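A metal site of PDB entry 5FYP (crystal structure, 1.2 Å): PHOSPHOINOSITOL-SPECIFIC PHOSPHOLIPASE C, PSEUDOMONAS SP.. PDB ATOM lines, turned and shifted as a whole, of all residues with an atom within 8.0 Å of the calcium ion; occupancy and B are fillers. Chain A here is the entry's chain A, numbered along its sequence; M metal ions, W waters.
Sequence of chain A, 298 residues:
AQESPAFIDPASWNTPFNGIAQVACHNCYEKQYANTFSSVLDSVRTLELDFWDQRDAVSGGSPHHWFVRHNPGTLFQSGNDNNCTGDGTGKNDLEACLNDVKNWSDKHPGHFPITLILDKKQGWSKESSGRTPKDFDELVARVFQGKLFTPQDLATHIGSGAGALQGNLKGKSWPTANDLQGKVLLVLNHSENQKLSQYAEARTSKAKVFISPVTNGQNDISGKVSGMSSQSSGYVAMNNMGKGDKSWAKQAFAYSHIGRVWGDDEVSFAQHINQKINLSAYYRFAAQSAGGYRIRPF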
ATOM      1  N   CYS A  25       6.173  21.225  -1.273  1.00  0.00           N
ATOM      2  CA  CYS A  25       6.958  20.403  -0.395  1.00  0.00           C
ATOM      3  C   CYS A  25       6.670  20.754   1.064  1.00  0.00           C
ATOM      4  O   CYS A  25       6.137  21.791   1.344  1.00  0.00           O
ATOM      5  CB  CYS A  25       8.459  20.544  -0.676  1.00  0.00           C
ATOM      6  SG  CYS A  25       9.274  21.861   0.215  1.00  0.00           S
ATOM      7  N   HIS A  26       7.088  19.885   1.973  1.00  0.00           N
ATOM      8  CA  HIS A  26       7.147  20.193   3.378  1.00  0.00           C
ATOM      9  C   HIS A  26       8.600  19.963   3.839  1.00  0.00           C
ATOM     10  O   HIS A  26       9.090  18.837   3.817  1.00  0.00           O
ATOM     11  CB  HIS A  26       6.177  19.339   4.178  1.00  0.00           C
ATOM     12  CG  HIS A  26       6.025  19.756   5.610  1.00  0.00           C
ATOM     13  ND1 HIS A  26       5.054  19.204   6.407  1.00  0.00           N
ATOM     14  CD2 HIS A  26       6.676  20.659   6.388  1.00  0.00           C
ATOM     15  CE1 HIS A  26       5.137  19.737   7.621  1.00  0.00           C
ATOM     16  NE2 HIS A  26       6.116  20.612   7.633  1.00  0.00           N
ATOM     17  N   ASN A  27       9.300  21.047   4.194  1.00  0.00           N
ATOM     18  CA  ASN A  27      10.662  20.944   4.698  1.00  0.00           C
ATOM     19  C   ASN A  27      11.617  20.266   3.728  1.00  0.00           C
ATOM     20  O   ASN A  27      12.551  19.550   4.131  1.00  0.00           O
ATOM     21  CB  ASN A  27      10.728  20.268   6.052  1.00  0.00           C
ATOM     22  CG  ASN A  27      10.166  21.123   7.169  1.00  0.00           C
ATOM     23  OD1 ASN A  27       9.763  22.267   6.990  1.00  0.00           O
ATOM     24  ND2 ASN A  27      10.069  20.528   8.288  1.00  0.00           N
ATOM     25  N   CYS A  28      11.471  20.551   2.430  1.00  0.00           N
ATOM     26  CA  CYS A  28      12.302  19.862   1.428  1.00  0.00           C
ATOM     27  C   CYS A  28      13.754  20.238   1.341  1.00  0.00           C
ATOM     28  O   CYS A  28      14.475  19.680   0.516  1.00  0.00           O
ATOM     29  CB  CYS A  28      11.685  19.920   0.045  1.00  0.00           C
ATOM     30  SG  CYS A  28      11.340  21.575  -0.556  1.00  0.00           S
ATOM     31  N   TYR A  29      14.175  21.180   2.181  1.00  0.00           N
ATOM     32  CA  TYR A  29      15.601  21.427   2.407  1.00  0.00           C
ATOM     33  C   TYR A  29      16.296  20.310   3.201  1.00  0.00           C
ATOM     34  O   TYR A  29      17.529  20.255   3.242  1.00  0.00           O
ATOM     35  CB  TYR A  29      15.757  22.768   3.171  1.00  0.00           C
ATOM     36  CG  TYR A  29      15.285  22.690   4.592  1.00  0.00           C
ATOM     37  CD1 TYR A  29      16.118  22.187   5.588  1.00  0.00           C
ATOM     38  CD2 TYR A  29      13.977  22.986   4.952  1.00  0.00           C
ATOM     39  CE1 TYR A  29      15.646  22.007   6.879  1.00  0.00           C
ATOM     40  CE2 TYR A  29      13.509  22.807   6.229  1.00  0.00           C
ATOM     41  CZ  TYR A  29      14.363  22.299   7.187  1.00  0.00           C
ATOM     42  OH  TYR A  29      13.914  22.053   8.475  1.00  0.00           O
ATOM     43  N   GLU A  30      15.539  19.448   3.854  1.00  0.00           N
ATOM     44  CA  GLU A  30      16.130  18.355   4.600  1.00  0.00           C
ATOM     45  C   GLU A  30      16.627  17.267   3.653  1.00  0.00           C
ATOM     46  O   GLU A  30      15.948  16.884   2.686  1.00  0.00           O
ATOM     47  CB  GLU A  30      15.170  17.764   5.622  1.00  0.00           C
ATOM     48  CG  GLU A  30      14.726  18.718   6.685  1.00  0.00           C
ATOM     49  CD  GLU A  30      13.945  18.031   7.790  1.00  0.00           C
ATOM     50  OE1 GLU A  30      14.532  17.105   8.401  1.00  0.00           O
ATOM     51  OE2 GLU A  30      12.792  18.403   8.039  1.00  0.00           O
ATOM     52  N   GLU A  48      10.288  25.093   0.622  1.00  0.00           N
ATOM     53  CA  GLU A  48      10.283  25.540   2.020  1.00  0.00           C
ATOM     54  C   GLU A  48      11.697  25.510   2.574  1.00  0.00           C
ATOM     55  O   GLU A  48      12.440  24.564   2.327  1.00  0.00           O
ATOM     56  CB  GLU A  48       9.376  24.653   2.884  1.00  0.00           C
ATOM     57  CG  GLU A  48       9.287  25.086   4.336  1.00  0.00           C
ATOM     58  CD  GLU A  48       8.203  24.394   5.129  1.00  0.00           C
ATOM     59  OE1 GLU A  48       7.691  23.360   4.657  1.00  0.00           O
ATOM     60  OE2 GLU A  48       7.876  24.882   6.240  1.00  0.00           O
ATOM     61  N   LEU A  49      12.010  26.529   3.360  1.00  0.00           N
ATOM     62  CA  LEU A  49      13.259  26.664   4.097  1.00  0.00           C
ATOM     63  C   LEU A  49      12.944  27.024   5.534  1.00  0.00           C
ATOM     64  O   LEU A  49      12.267  28.024   5.766  1.00  0.00           O
ATOM     65  CB  LEU A  49      14.162  27.744   3.477  1.00  0.00           C
ATOM     66  CG  LEU A  49      14.702  27.407   2.099  1.00  0.00           C
ATOM     67  CD1 LEU A  49      15.147  28.622   1.338  1.00  0.00           C
ATOM     68  CD2 LEU A  49      15.833  26.379   2.218  1.00  0.00           C
ATOM     69  N   ASP A  50      13.514  26.279   6.495  1.00  0.00           N
ATOM     70  CA  ASP A  50      13.450  26.666   7.909  1.00  0.00           C
ATOM     71  C   ASP A  50      14.732  27.412   8.243  1.00  0.00           C
ATOM     72  O   ASP A  50      15.837  26.881   7.995  1.00  0.00           O
ATOM     73  CB  ASP A  50      13.362  25.434   8.812  1.00  0.00           C
ATOM     74  CG  ASP A  50      12.035  24.687   8.731  1.00  0.00           C
ATOM     75  OD1 ASP A  50      11.090  25.186   8.115  1.00  0.00           O
ATOM     76  OD2 ASP A  50      11.969  23.574   9.304  1.00  0.00           O
ATOM     77  N   PHE A  51      14.610  28.615   8.816  1.00  0.00           N
ATOM     78  CA  PHE A  51      15.816  29.424   8.988  1.00  0.00           C
ATOM     79  C   PHE A  51      15.951  29.969  10.397  1.00  0.00           C
ATOM     80  O   PHE A  51      14.985  30.397  11.042  1.00  0.00           O
ATOM     81  CB  PHE A  51      15.932  30.509   7.902  1.00  0.00           C
ATOM     82  CG  PHE A  51      14.958  31.664   8.024  1.00  0.00           C
ATOM     83  CD1 PHE A  51      13.645  31.591   7.565  1.00  0.00           C
ATOM     84  CD2 PHE A  51      15.395  32.882   8.523  1.00  0.00           C
ATOM     85  CE1 PHE A  51      12.799  32.686   7.629  1.00  0.00           C
ATOM     86  CE2 PHE A  51      14.561  33.972   8.576  1.00  0.00           C
ATOM     87  CZ  PHE A  51      13.265  33.879   8.137  1.00  0.00           C
ATOM     88  N   ARG A  69      18.277  24.707   8.834  1.00  0.00           N
ATOM     89  CA  ARG A  69      18.254  23.389   9.473  1.00  0.00           C
ATOM     90  C   ARG A  69      16.880  23.196  10.112  1.00  0.00           C
ATOM     91  O   ARG A  69      16.132  24.177  10.291  1.00  0.00           O
ATOM     92  CB  ARG A  69      19.326  23.250  10.544  1.00  0.00           C
ATOM     93  CG  ARG A  69      19.115  24.169  11.746  1.00  0.00           C
ATOM     94  CD  ARG A  69      20.164  23.898  12.820  1.00  0.00           C
ATOM     95  NE  ARG A  69      19.963  24.759  13.993  1.00  0.00           N
ATOM     96  CZ  ARG A  69      20.346  26.016  14.076  1.00  0.00           C
ATOM     97  NH1 ARG A  69      21.070  26.577  13.111  1.00  0.00           N
ATOM     98  NH2 ARG A  69      19.989  26.748  15.142  1.00  0.00           N
ATOM     99  N   HIS A  70      16.603  21.967  10.524  1.00  0.00           N
ATOM    100  CA  HIS A  70      15.330  21.684  11.154  1.00  0.00           C
ATOM    101  C   HIS A  70      15.330  21.931  12.672  1.00  0.00           C
ATOM    102  O   HIS A  70      14.431  22.589  13.184  1.00  0.00           O
ATOM    103  CB  HIS A  70      14.917  20.252  10.862  1.00  0.00           C
ATOM    104  CG  HIS A  70      13.532  19.903  11.335  1.00  0.00           C
ATOM    105  ND1 HIS A  70      13.289  18.998  12.321  1.00  0.00           N
ATOM    106  CD2 HIS A  70      12.325  20.416  11.008  1.00  0.00           C
ATOM    107  CE1 HIS A  70      11.994  18.896  12.535  1.00  0.00           C
ATOM    108  NE2 HIS A  70      11.381  19.761  11.765  1.00  0.00           N
ATOM    109  N   ILE A 117       8.398  29.196   0.889  1.00  0.00           N
ATOM    110  CA  ILE A 117       7.931  29.353   2.262  1.00  0.00           C
ATOM    111  C   ILE A 117       9.161  29.439   3.154  1.00  0.00           C
ATOM    112  O   ILE A 117       9.964  28.523   3.233  1.00  0.00           O
ATOM    113  CB  ILE A 117       7.068  28.132   2.681  1.00  0.00           C
ATOM    114  CG1 ILE A 117       5.913  27.875   1.656  1.00  0.00           C
ATOM    115  CG2 ILE A 117       6.570  28.259   4.116  1.00  0.00           C
ATOM    116  CD1 ILE A 117       4.958  29.012   1.412  1.00  0.00           C
ATOM    117  N   LEU A 118       9.328  30.601   3.796  1.00  0.00           N
ATOM    118  CA  LEU A 118      10.452  30.900   4.671  1.00  0.00           C
ATOM    119  C   LEU A 118       9.923  30.808   6.103  1.00  0.00           C
ATOM    120  O   LEU A 118       9.276  31.737   6.587  1.00  0.00           O
ATOM    121  CB  LEU A 118      11.041  32.250   4.318  1.00  0.00           C
ATOM    122  CG  LEU A 118      11.449  32.407   2.843  1.00  0.00           C
ATOM    123  CD1 LEU A 118      11.925  33.812   2.582  1.00  0.00           C
ATOM    124  CD2 LEU A 118      12.474  31.396   2.416  1.00  0.00           C
ATOM    125  N   ASP A 119      10.195  29.675   6.731  1.00  0.00           N
ATOM    126  CA  ASP A 119       9.657  29.337   8.039  1.00  0.00           C
ATOM    127  C   ASP A 119      10.698  29.736   9.092  1.00  0.00           C
ATOM    128  O   ASP A 119      11.708  29.090   9.299  1.00  0.00           O
ATOM    129  CB  ASP A 119       9.325  27.858   8.090  1.00  0.00           C
ATOM    130  CG  ASP A 119       8.536  27.425   9.307  1.00  0.00           C
ATOM    131  OD1 ASP A 119       8.084  28.319  10.060  1.00  0.00           O
ATOM    132  OD2 ASP A 119       8.347  26.170   9.471  1.00  0.00           O
ATOM    133  N   LYS A 120      10.456  30.919   9.686  1.00  0.00           N
ATOM    134  CA  LYS A 120      11.386  31.533  10.601  1.00  0.00           C
ATOM    135  C   LYS A 120      11.289  30.864  11.969  1.00  0.00           C
ATOM    136  O   LYS A 120      10.204  30.712  12.494  1.00  0.00           O
ATOM    137  CB  LYS A 120      11.068  33.021  10.730  1.00  0.00           C
ATOM    138  CG  LYS A 120      12.147  33.779  11.482  1.00  0.00           C
ATOM    139  CD  LYS A 120      11.896  35.277  11.551  1.00  0.00           C
ATOM    140  CE  LYS A 120      13.109  36.123  11.771  1.00  0.00           C
ATOM    141  NZ  LYS A 120      14.124  35.591  12.712  1.00  0.00           N
ATOM    142  N   LYS A 121      12.439  30.518  12.545  1.00  0.00           N
ATOM    143  CA  LYS A 121      12.468  29.702  13.777  1.00  0.00           C
ATOM    144  C   LYS A 121      12.848  30.444  15.049  1.00  0.00           C
ATOM    145  O   LYS A 121      12.626  29.914  16.138  1.00  0.00           O
ATOM    146  CB  LYS A 121      13.359  28.485  13.559  1.00  0.00           C
ATOM    147  CG  LYS A 121      12.821  27.540  12.489  1.00  0.00           C
ATOM    148  CD  LYS A 121      11.505  26.896  12.846  1.00  0.00           C
ATOM    149  CE  LYS A 121      10.950  26.042  11.736  1.00  0.00           C
ATOM    150  NZ  LYS A 121       9.638  25.450  12.097  1.00  0.00           N
ATOM    151  N   ASN A 189       6.564  32.521   7.433  1.00  0.00           N
ATOM    152  CA  ASN A 189       5.833  31.810   8.478  1.00  0.00           C
ATOM    153  C   ASN A 189       6.631  31.911   9.777  1.00  0.00           C
ATOM    154  O   ASN A 189       7.854  32.116   9.759  1.00  0.00           O
ATOM    155  CB  ASN A 189       5.608  30.325   8.132  1.00  0.00           C
ATOM    156  CG  ASN A 189       4.676  30.058   6.971  1.00  0.00           C
ATOM    157  OD1 ASN A 189       3.948  30.928   6.432  1.00  0.00           O
ATOM    158  ND2 ASN A 189       4.632  28.843   6.604  1.00  0.00           N
ATOM    159  N   ASN A 240      -1.829  30.416   6.672  1.00  0.00           N
ATOM    160  CA  ASN A 240      -1.123  29.164   6.944  1.00  0.00           C
ATOM    161  C   ASN A 240      -1.935  28.353   7.953  1.00  0.00           C
ATOM    162  O   ASN A 240      -2.254  28.813   9.043  1.00  0.00           O
ATOM    163  CB  ASN A 240       0.334  29.357   7.423  1.00  0.00           C
ATOM    164  CG  ASN A 240       1.296  28.193   7.023  1.00  0.00           C
ATOM    165  OD1 ASN A 240       1.476  27.739   5.859  1.00  0.00           O
ATOM    166  ND2 ASN A 240       2.002  27.769   8.040  1.00  0.00           N
ATOM    167  N   ARG A 260      -2.167  27.776   2.546  1.00  0.00           N
ATOM    168  CA  ARG A 260      -1.269  26.610   2.607  1.00  0.00           C
ATOM    169  C   ARG A 260      -1.702  25.732   3.771  1.00  0.00           C
ATOM    170  O   ARG A 260      -1.980  26.240   4.869  1.00  0.00           O
ATOM    171  CB  ARG A 260       0.168  27.038   2.793  1.00  0.00           C
ATOM    172  CG  ARG A 260       1.164  25.883   2.834  1.00  0.00           C
ATOM    173  CD  ARG A 260       2.591  26.372   2.565  1.00  0.00           C
ATOM    174  NE  ARG A 260       3.614  25.328   2.627  1.00  0.00           N
ATOM    175  CZ  ARG A 260       4.123  24.885   3.744  1.00  0.00           C
ATOM    176  NH1 ARG A 260       3.642  25.283   4.914  1.00  0.00           N
ATOM    177  NH2 ARG A 260       5.113  23.981   3.682  1.00  0.00           N
ATOM    178  N   TRP A 262      -0.397  22.316   5.871  1.00  0.00           N
ATOM    179  CA  TRP A 262       0.702  21.414   6.163  1.00  0.00           C
ATOM    180  C   TRP A 262       0.254  20.346   7.158  1.00  0.00           C
ATOM    181  O   TRP A 262      -0.696  20.550   7.911  1.00  0.00           O
ATOM    182  CB  TRP A 262       1.923  22.193   6.672  1.00  0.00           C
ATOM    183  CG  TRP A 262       1.651  23.006   7.895  1.00  0.00           C
ATOM    184  CD1 TRP A 262       1.187  24.266   7.961  1.00  0.00           C
ATOM    185  CD2 TRP A 262       1.811  22.554   9.243  1.00  0.00           C
ATOM    186  NE1 TRP A 262       1.014  24.640   9.280  1.00  0.00           N
ATOM    187  CE2 TRP A 262       1.411  23.606  10.078  1.00  0.00           C
ATOM    188  CE3 TRP A 262       2.264  21.362   9.822  1.00  0.00           C
ATOM    189  CZ2 TRP A 262       1.440  23.498  11.479  1.00  0.00           C
ATOM    190  CZ3 TRP A 262       2.292  21.249  11.215  1.00  0.00           C
ATOM    191  CH2 TRP A 262       1.878  22.322  12.017  1.00  0.00           C
ATOM    192  N   TYR A 283       5.573  15.955   2.663  1.00  0.00           N
ATOM    193  CA  TYR A 283       6.948  15.466   2.762  1.00  0.00           C
ATOM    194  C   TYR A 283       7.372  14.767   1.466  1.00  0.00           C
ATOM    195  O   TYR A 283       8.444  15.021   0.919  1.00  0.00           O
ATOM    196  CB  TYR A 283       7.094  14.533   3.938  1.00  0.00           C
ATOM    197  CG  TYR A 283       6.847  15.191   5.259  1.00  0.00           C
ATOM    198  CD1 TYR A 283       7.721  16.171   5.740  1.00  0.00           C
ATOM    199  CD2 TYR A 283       5.771  14.821   6.082  1.00  0.00           C
ATOM    200  CE1 TYR A 283       7.531  16.760   6.980  1.00  0.00           C
ATOM    201  CE2 TYR A 283       5.557  15.425   7.308  1.00  0.00           C
ATOM    202  CZ  TYR A 283       6.452  16.376   7.765  1.00  0.00           C
ATOM    203  OH  TYR A 283       6.297  16.957   9.001  1.00  0.00           O
HETATM  204 CA    CA M   1       8.999  24.188   8.234  1.00  0.00          CA
HETATM  205  O   HOH W   1       6.994  23.065   8.909  1.00  0.00           O
HETATM  206  O   HOH W   2       9.502  23.066  10.318  1.00  0.00           O
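Water W2 lies within hydrogen-bond range of the side-chain carboxylate (OD2) of Asp 50 (2.7 Å), the side-chain amino group (NZ) of Lys 121 (3.0 Å) and the side-chain amide nitrogen (ND2) of Asn 27 (3.3 Å).
OD2 of Asp 50 is in hydrogen-bond range of OH of Tyr 29, 2.6 Å away.
The backbone NH of Arg 69 sits at hydrogen-bond distance from the backbone carbonyl oxygen of Asp 50, at 3.4 Å.
The side-chain carboxylate of Glu 48 lies within salt-bridge range of the guanidinium group of Arg 260 (2.8 Å).
The side-chain sulfur (SG) of Cys 25 sits at hydrogen-bond distance from the backbone NH (N) of Glu 48, 3.4 Å away.
The side-chain amide nitrogen (ND2) of Asn 27 sits close to the side-chain carboxylate (OE2) of Glu 30, at 3.5 Å.
The side-chain amino group (NZ) of Lys 121 lies within salt-bridge range of the side-chain carboxylate (OD1) of Asp 119, at 3.8 Å.
The backbone carbonyl oxygen (O) of Asp 119 lies within hydrogen-bond range of the backbone NH (N) of Phe 51, at 3.0 Å.
The side-chain sulfur (SG) of Cys 25 forms a disulfide with the side-chain sulfur (SG) of Cys 28, at 2.2 Å.
The calcium ion is bound by the side-chain carboxylate (OD1) of Asp 50 (2.3 Å), the side-chain carboxylate (OE2) of Glu 48 (2.4 Å), water W1 (2.4 Å), the side-chain amide oxygen (OD1) of Asn 27 (2.4 Å), water W2 (2.4 Å) and the side-chain carboxylate (OD2) of Asp 119 (2.4 Å).
The calcium ion has six donor atoms within binding distance.
Of the 22 residues printed, 4 come within 4 Å of the calcium ion.
The nearest printed residue that does not touch the calcium ion is Lys 121 (4.1 Å).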
